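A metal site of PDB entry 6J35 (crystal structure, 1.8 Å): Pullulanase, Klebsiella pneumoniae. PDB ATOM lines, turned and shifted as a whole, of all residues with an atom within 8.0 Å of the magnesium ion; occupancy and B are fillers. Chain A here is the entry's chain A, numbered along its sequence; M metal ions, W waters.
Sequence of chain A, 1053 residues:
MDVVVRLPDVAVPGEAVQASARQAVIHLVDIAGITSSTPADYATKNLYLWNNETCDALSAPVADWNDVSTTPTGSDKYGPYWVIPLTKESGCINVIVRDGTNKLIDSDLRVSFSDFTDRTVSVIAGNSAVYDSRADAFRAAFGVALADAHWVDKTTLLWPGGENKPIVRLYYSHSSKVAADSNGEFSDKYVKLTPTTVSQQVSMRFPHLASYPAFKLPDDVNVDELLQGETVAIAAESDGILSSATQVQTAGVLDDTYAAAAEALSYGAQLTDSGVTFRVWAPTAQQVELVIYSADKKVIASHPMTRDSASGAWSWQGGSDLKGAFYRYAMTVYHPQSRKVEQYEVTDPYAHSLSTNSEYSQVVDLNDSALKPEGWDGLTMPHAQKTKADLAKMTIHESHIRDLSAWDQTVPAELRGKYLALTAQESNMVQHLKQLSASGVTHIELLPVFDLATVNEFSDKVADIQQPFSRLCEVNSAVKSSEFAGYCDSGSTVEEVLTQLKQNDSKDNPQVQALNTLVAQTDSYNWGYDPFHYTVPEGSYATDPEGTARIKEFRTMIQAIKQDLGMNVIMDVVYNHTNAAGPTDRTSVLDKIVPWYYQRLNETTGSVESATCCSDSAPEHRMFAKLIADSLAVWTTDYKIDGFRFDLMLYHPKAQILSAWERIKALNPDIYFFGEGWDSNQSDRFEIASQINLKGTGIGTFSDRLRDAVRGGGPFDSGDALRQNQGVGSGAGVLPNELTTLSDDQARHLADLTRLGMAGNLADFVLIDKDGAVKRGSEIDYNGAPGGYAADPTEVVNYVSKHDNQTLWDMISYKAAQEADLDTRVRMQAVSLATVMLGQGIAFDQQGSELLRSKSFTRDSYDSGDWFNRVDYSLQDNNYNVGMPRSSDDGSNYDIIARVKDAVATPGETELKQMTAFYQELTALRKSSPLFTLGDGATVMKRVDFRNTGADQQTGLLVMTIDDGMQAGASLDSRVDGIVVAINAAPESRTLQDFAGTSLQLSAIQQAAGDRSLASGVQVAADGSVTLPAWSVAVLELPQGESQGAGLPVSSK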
ATOM      1  N   SER A 929      -1.372 -22.981  18.632  1.00  0.00           N
ATOM      2  CA  SER A 929      -0.859 -22.445  19.908  1.00  0.00           C
ATOM      3  C   SER A 929       0.646 -22.636  20.001  1.00  0.00           C
ATOM      4  O   SER A 929       1.162 -23.712  19.663  1.00  0.00           O
ATOM      5  CB  SER A 929      -1.517 -23.116  21.116  1.00  0.00           C
ATOM      6  OG  SER A 929      -0.958 -22.641  22.338  1.00  0.00           O
ATOM      7  N   PRO A 930       1.377 -21.630  20.471  1.00  0.00           N
ATOM      8  CA  PRO A 930       2.809 -21.810  20.736  1.00  0.00           C
ATOM      9  C   PRO A 930       3.136 -22.794  21.853  1.00  0.00           C
ATOM     10  O   PRO A 930       4.315 -23.156  22.008  1.00  0.00           O
ATOM     11  CB  PRO A 930       3.270 -20.387  21.111  1.00  0.00           C
ATOM     12  CG  PRO A 930       2.063 -19.725  21.654  1.00  0.00           C
ATOM     13  CD  PRO A 930       0.928 -20.253  20.775  1.00  0.00           C
ATOM     14  N   LEU A 931       2.159 -23.209  22.667  1.00  0.00           N
ATOM     15  CA  LEU A 931       2.476 -24.169  23.722  1.00  0.00           C
ATOM     16  C   LEU A 931       2.853 -25.539  23.145  1.00  0.00           C
ATOM     17  O   LEU A 931       3.564 -26.307  23.804  1.00  0.00           O
ATOM     18  CB  LEU A 931       1.298 -24.274  24.705  1.00  0.00           C
ATOM     19  CG  LEU A 931       0.923 -22.958  25.393  1.00  0.00           C
ATOM     20  CD1 LEU A 931      -0.432 -23.056  26.085  1.00  0.00           C
ATOM     21  CD2 LEU A 931       2.000 -22.545  26.393  1.00  0.00           C
ATOM     22  N   ARG A 943       7.231 -26.606  31.772  1.00  0.00           N
ATOM     23  CA  ARG A 943       5.814 -26.512  31.417  1.00  0.00           C
ATOM     24  C   ARG A 943       5.139 -27.845  31.114  1.00  0.00           C
ATOM     25  O   ARG A 943       3.918 -27.927  31.258  1.00  0.00           O
ATOM     26  CB  ARG A 943       5.623 -25.580  30.209  1.00  0.00           C
ATOM     27  CG  ARG A 943       6.019 -24.124  30.453  1.00  0.00           C
ATOM     28  CD  ARG A 943       5.863 -23.280  29.178  1.00  0.00           C
ATOM     29  NE  ARG A 943       6.220 -21.883  29.423  1.00  0.00           N
ATOM     30  CZ  ARG A 943       5.368 -20.868  29.501  1.00  0.00           C
ATOM     31  NH1 ARG A 943       4.076 -21.056  29.317  1.00  0.00           N
ATOM     32  NH2 ARG A 943       5.811 -19.627  29.711  1.00  0.00           N
ATOM     33  N   ASP A 963       1.770 -26.229  30.603  1.00  0.00           N
ATOM     34  CA  ASP A 963       1.406 -25.113  31.465  1.00  0.00           C
ATOM     35  C   ASP A 963       1.589 -23.777  30.748  1.00  0.00           C
ATOM     36  O   ASP A 963       2.629 -23.542  30.121  1.00  0.00           O
ATOM     37  CB  ASP A 963       2.282 -25.171  32.718  1.00  0.00           C
ATOM     38  CG  ASP A 963       1.795 -24.273  33.833  1.00  0.00           C
ATOM     39  OD1 ASP A 963       0.665 -23.735  33.754  1.00  0.00           O
ATOM     40  OD2 ASP A 963       2.580 -24.129  34.801  1.00  0.00           O
ATOM     41  N   ASP A 964       0.581 -22.904  30.832  1.00  0.00           N
ATOM     42  CA  ASP A 964       0.782 -21.497  30.512  1.00  0.00           C
ATOM     43  C   ASP A 964       0.472 -20.585  31.706  1.00  0.00           C
ATOM     44  O   ASP A 964       0.328 -19.368  31.515  1.00  0.00           O
ATOM     45  CB  ASP A 964      -0.050 -21.064  29.296  1.00  0.00           C
ATOM     46  CG  ASP A 964       0.583 -19.894  28.535  1.00  0.00           C
ATOM     47  OD1 ASP A 964       1.833 -19.806  28.494  1.00  0.00           O
ATOM     48  OD2 ASP A 964      -0.167 -19.038  27.989  1.00  0.00           O
ATOM     49  N   GLY A 965       0.354 -21.154  32.917  1.00  0.00           N
ATOM     50  CA  GLY A 965      -0.010 -20.376  34.088  1.00  0.00           C
ATOM     51  C   GLY A 965       1.171 -19.742  34.811  1.00  0.00           C
ATOM     52  O   GLY A 965       2.336 -19.858  34.427  1.00  0.00           O
ATOM     53  N   ALA A 970       5.804 -16.413  31.785  1.00  0.00           N
ATOM     54  CA  ALA A 970       4.872 -15.540  31.103  1.00  0.00           C
ATOM     55  C   ALA A 970       3.851 -16.346  30.318  1.00  0.00           C
ATOM     56  O   ALA A 970       4.085 -17.495  29.942  1.00  0.00           O
ATOM     57  CB  ALA A 970       5.626 -14.588  30.162  1.00  0.00           C
ATOM     58  N   SER A 971       2.709 -15.729  30.065  1.00  0.00           N
ATOM     59  CA  SER A 971       1.720 -16.329  29.171  1.00  0.00           C
ATOM     60  C   SER A 971       2.227 -16.228  27.737  1.00  0.00           C
ATOM     61  O   SER A 971       2.483 -15.134  27.238  1.00  0.00           O
ATOM     62  CB  SER A 971       0.375 -15.607  29.325  1.00  0.00           C
ATOM     63  OG  SER A 971      -0.563 -15.996  28.334  1.00  0.00           O
ATOM     64  N   LEU A 972       2.401 -17.386  27.095  1.00  0.00           N
ATOM     65  CA  LEU A 972       2.801 -17.444  25.695  1.00  0.00           C
ATOM     66  C   LEU A 972       1.611 -17.418  24.753  1.00  0.00           C
ATOM     67  O   LEU A 972       1.807 -17.199  23.551  1.00  0.00           O
ATOM     68  CB  LEU A 972       3.613 -18.712  25.450  1.00  0.00           C
ATOM     69  CG  LEU A 972       4.845 -18.903  26.317  1.00  0.00           C
ATOM     70  CD1 LEU A 972       5.469 -20.246  25.963  1.00  0.00           C
ATOM     71  CD2 LEU A 972       5.822 -17.760  26.045  1.00  0.00           C
ATOM     72  N   ASP A 973       0.407 -17.598  25.274  1.00  0.00           N
ATOM     73  CA  ASP A 973      -0.802 -17.755  24.477  1.00  0.00           C
ATOM     74  C   ASP A 973      -1.897 -17.017  25.236  1.00  0.00           C
ATOM     75  O   ASP A 973      -2.298 -17.460  26.327  1.00  0.00           O
ATOM     76  CB  ASP A 973      -1.123 -19.248  24.298  1.00  0.00           C
ATOM     77  CG  ASP A 973      -2.333 -19.518  23.408  1.00  0.00           C
ATOM     78  OD1 ASP A 973      -3.130 -18.598  23.119  1.00  0.00           O
ATOM     79  OD2 ASP A 973      -2.475 -20.696  23.004  1.00  0.00           O
ATOM     80  N   SER A 974      -2.362 -15.890  24.705  1.00  0.00           N
ATOM     81  CA  SER A 974      -3.328 -15.080  25.440  1.00  0.00           C
ATOM     82  C   SER A 974      -4.689 -15.740  25.581  1.00  0.00           C
ATOM     83  O   SER A 974      -5.503 -15.298  26.404  1.00  0.00           O
ATOM     84  CB  SER A 974      -3.480 -13.708  24.745  1.00  0.00           C
ATOM     85  OG  SER A 974      -4.055 -13.865  23.464  1.00  0.00           O
ATOM     86  N   ARG A 975      -4.978 -16.781  24.798  1.00  0.00           N
ATOM     87  CA  ARG A 975      -6.294 -17.400  24.831  1.00  0.00           C
ATOM     88  C   ARG A 975      -6.441 -18.462  25.897  1.00  0.00           C
ATOM     89  O   ARG A 975      -7.566 -18.736  26.306  1.00  0.00           O
ATOM     90  CB  ARG A 975      -6.624 -18.017  23.465  1.00  0.00           C
ATOM     91  CG  ARG A 975      -6.646 -16.994  22.345  1.00  0.00           C
ATOM     92  CD  ARG A 975      -7.378 -17.481  21.118  1.00  0.00           C
ATOM     93  NE  ARG A 975      -7.287 -16.516  20.023  1.00  0.00           N
ATOM     94  CZ  ARG A 975      -7.862 -16.682  18.836  1.00  0.00           C
ATOM     95  NH1 ARG A 975      -7.744 -15.749  17.896  1.00  0.00           N
ATOM     96  NH2 ARG A 975      -8.577 -17.797  18.596  1.00  0.00           N
ATOM     97  N   VAL A 976      -5.351 -19.073  26.368  1.00  0.00           N
ATOM     98  CA  VAL A 976      -5.446 -20.214  27.273  1.00  0.00           C
ATOM     99  C   VAL A 976      -4.388 -20.096  28.362  1.00  0.00           C
ATOM    100  O   VAL A 976      -3.339 -19.469  28.184  1.00  0.00           O
ATOM    101  CB  VAL A 976      -5.289 -21.585  26.568  1.00  0.00           C
ATOM    102  CG1 VAL A 976      -6.242 -21.718  25.375  1.00  0.00           C
ATOM    103  CG2 VAL A 976      -3.849 -21.836  26.141  1.00  0.00           C
ATOM    104  N   ASP A 977      -4.675 -20.756  29.485  1.00  0.00           N
ATOM    105  CA  ASP A 977      -3.766 -20.895  30.624  1.00  0.00           C
ATOM    106  C   ASP A 977      -3.103 -22.258  30.662  1.00  0.00           C
ATOM    107  O   ASP A 977      -2.295 -22.524  31.558  1.00  0.00           O
ATOM    108  CB  ASP A 977      -4.523 -20.668  31.935  1.00  0.00           C
ATOM    109  CG  ASP A 977      -4.786 -19.196  32.219  1.00  0.00           C
ATOM    110  OD1 ASP A 977      -3.927 -18.343  31.903  1.00  0.00           O
ATOM    111  OD2 ASP A 977      -5.863 -18.891  32.779  1.00  0.00           O
ATOM    112  N   GLY A 978      -3.424 -23.123  29.723  1.00  0.00           N
ATOM    113  CA  GLY A 978      -2.864 -24.453  29.714  1.00  0.00           C
ATOM    114  C   GLY A 978      -3.581 -25.335  28.712  1.00  0.00           C
ATOM    115  O   GLY A 978      -4.692 -25.011  28.282  1.00  0.00           O
ATOM    116  N   LEU A1038      -7.577 -24.598  29.200  1.00  0.00           N
ATOM    117  CA  LEU A1038      -8.071 -23.740  30.255  1.00  0.00           C
ATOM    118  C   LEU A1038      -8.230 -22.346  29.679  1.00  0.00           C
ATOM    119  O   LEU A1038      -7.219 -21.708  29.348  1.00  0.00           O
ATOM    120  CB  LEU A1038      -7.091 -23.725  31.431  1.00  0.00           C
ATOM    121  CG  LEU A1038      -6.885 -25.047  32.181  1.00  0.00           C
ATOM    122  CD1 LEU A1038      -5.796 -24.892  33.225  1.00  0.00           C
ATOM    123  CD2 LEU A1038      -8.199 -25.531  32.829  1.00  0.00           C
ATOM    124  N   PRO A1039      -9.445 -21.826  29.519  1.00  0.00           N
ATOM    125  CA  PRO A1039      -9.603 -20.492  28.922  1.00  0.00           C
ATOM    126  C   PRO A1039      -8.963 -19.420  29.801  1.00  0.00           C
ATOM    127  O   PRO A1039      -9.096 -19.445  31.019  1.00  0.00           O
ATOM    128  CB  PRO A1039     -11.129 -20.306  28.862  1.00  0.00           C
ATOM    129  CG  PRO A1039     -11.640 -21.172  29.972  1.00  0.00           C
ATOM    130  CD  PRO A1039     -10.730 -22.373  29.993  1.00  0.00           C
ATOM    131  N   GLN A1040      -8.269 -18.468  29.158  1.00  0.00           N
ATOM    132  CA  GLN A1040      -7.583 -17.425  29.918  1.00  0.00           C
ATOM    133  C   GLN A1040      -8.510 -16.231  30.113  1.00  0.00           C
ATOM    134  O   GLN A1040      -9.183 -15.801  29.165  1.00  0.00           O
ATOM    135  CB  GLN A1040      -6.305 -16.977  29.218  1.00  0.00           C
ATOM    136  CG  GLN A1040      -5.426 -16.032  30.046  1.00  0.00           C
ATOM    137  CD  GLN A1040      -4.074 -15.799  29.401  1.00  0.00           C
ATOM    138  OE1 GLN A1040      -3.579 -16.675  28.679  1.00  0.00           O
ATOM    139  NE2 GLN A1040      -3.477 -14.636  29.635  1.00  0.00           N
ATOM    140  N   GLY A1041      -8.560 -15.725  31.338  1.00  0.00           N
ATOM    141  CA  GLY A1041      -9.441 -14.626  31.688  1.00  0.00           C
ATOM    142  C   GLY A1041      -8.715 -13.300  31.734  1.00  0.00           C
ATOM    143  O   GLY A1041      -7.793 -13.042  30.952  1.00  0.00           O
ATOM    144  N   SER A1043      -6.594 -11.948  33.846  1.00  0.00           N
ATOM    145  CA  SER A1043      -5.167 -12.107  34.027  1.00  0.00           C
ATOM    146  C   SER A1043      -4.774 -13.556  33.806  1.00  0.00           C
ATOM    147  O   SER A1043      -5.610 -14.466  33.863  1.00  0.00           O
ATOM    148  CB  SER A1043      -4.728 -11.690  35.450  1.00  0.00           C
ATOM    149  OG  SER A1043      -5.301 -10.457  35.829  1.00  0.00           O
ATOM    150  N   GLN A1044      -3.481 -13.776  33.592  1.00  0.00           N
ATOM    151  CA  GLN A1044      -2.942 -15.116  33.603  1.00  0.00           C
ATOM    152  C   GLN A1044      -3.392 -15.867  34.857  1.00  0.00           C
ATOM    153  O   GLN A1044      -3.386 -15.312  35.971  1.00  0.00           O
ATOM    154  CB  GLN A1044      -1.416 -15.055  33.517  1.00  0.00           C
ATOM    155  CG  GLN A1044      -0.719 -16.402  33.555  1.00  0.00           C
ATOM    156  CD  GLN A1044       0.791 -16.280  33.529  1.00  0.00           C
ATOM    157  OE1 GLN A1044       1.369 -15.418  34.188  1.00  0.00           O
ATOM    158  NE2 GLN A1044       1.435 -17.162  32.781  1.00  0.00           N
ATOM    159  N   GLY A1045      -3.792 -17.127  34.683  1.00  0.00           N
ATOM    160  CA  GLY A1045      -4.330 -17.936  35.750  1.00  0.00           C
ATOM    161  C   GLY A1045      -3.371 -18.989  36.273  1.00  0.00           C
ATOM    162  O   GLY A1045      -2.170 -18.980  36.006  1.00  0.00           O
HETATM  163 MG    MG M   1      -1.884 -17.877  28.323  1.00  0.00          MG
HETATM  164  O   HOH W   1      -1.732 -17.994  30.412  1.00  0.00           O
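The magnesium ion is bound by O of Asp 973, 2.1 Å away.
The magnesium ion is bound by water W1 (2.1 Å).
OD2 of Asp 964 binds the magnesium ion, at 2.1 Å.
The side-chain amide oxygen (OE1) of Gln 1040 binds the magnesium ion (2.1 Å).
The magnesium ion is bound by the backbone carbonyl oxygen (O) of Val 976, at 2.2 Å.
The magnesium ion is bound by OG of Ser 971 (2.3 Å).
The magnesium ion has six donor atoms within binding distance.
Of the 23 residues printed, 5 come within 4 Å of the magnesium ion.
N of Arg 975 is in hydrogen-bond range of OD1 of Asp 973, at 3.1 Å.
The side-chain carboxylate (OD2) of Asp 973 lies within hydrogen-bond range of the side-chain hydroxyl (OG) of Ser 929, at 2.6 Å.
O of Asp 977 lies within hydrogen-bond range of N of Asp 964 (3.0 Å).
The side-chain carboxylate (OD1) of Asp 964 is in hydrogen-bond range of the backbone NH (N) of Leu 972 (2.9 Å).
The backbone carbonyl oxygen (O) of Asp 964 lies within hydrogen-bond range of the side-chain amide nitrogen (NE2) of Gln 1044 (2.8 Å).
OE1 of Gln 1040 sits close to O of Ser 974, 3.3 Å away.
O of Arg 975 lies within hydrogen-bond range of N of Gln 1040, at 2.9 Å.
The backbone NH (N) of Ser 971 lies close to the side-chain amide nitrogen (NE2) of Gln 1044, at 3.3 Å.
Water W1 lies within hydrogen-bond range of the side-chain carboxylate of Asp 977 (2.7 Å) and the backbone carbonyl oxygen of Asp 964 (2.7 Å).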
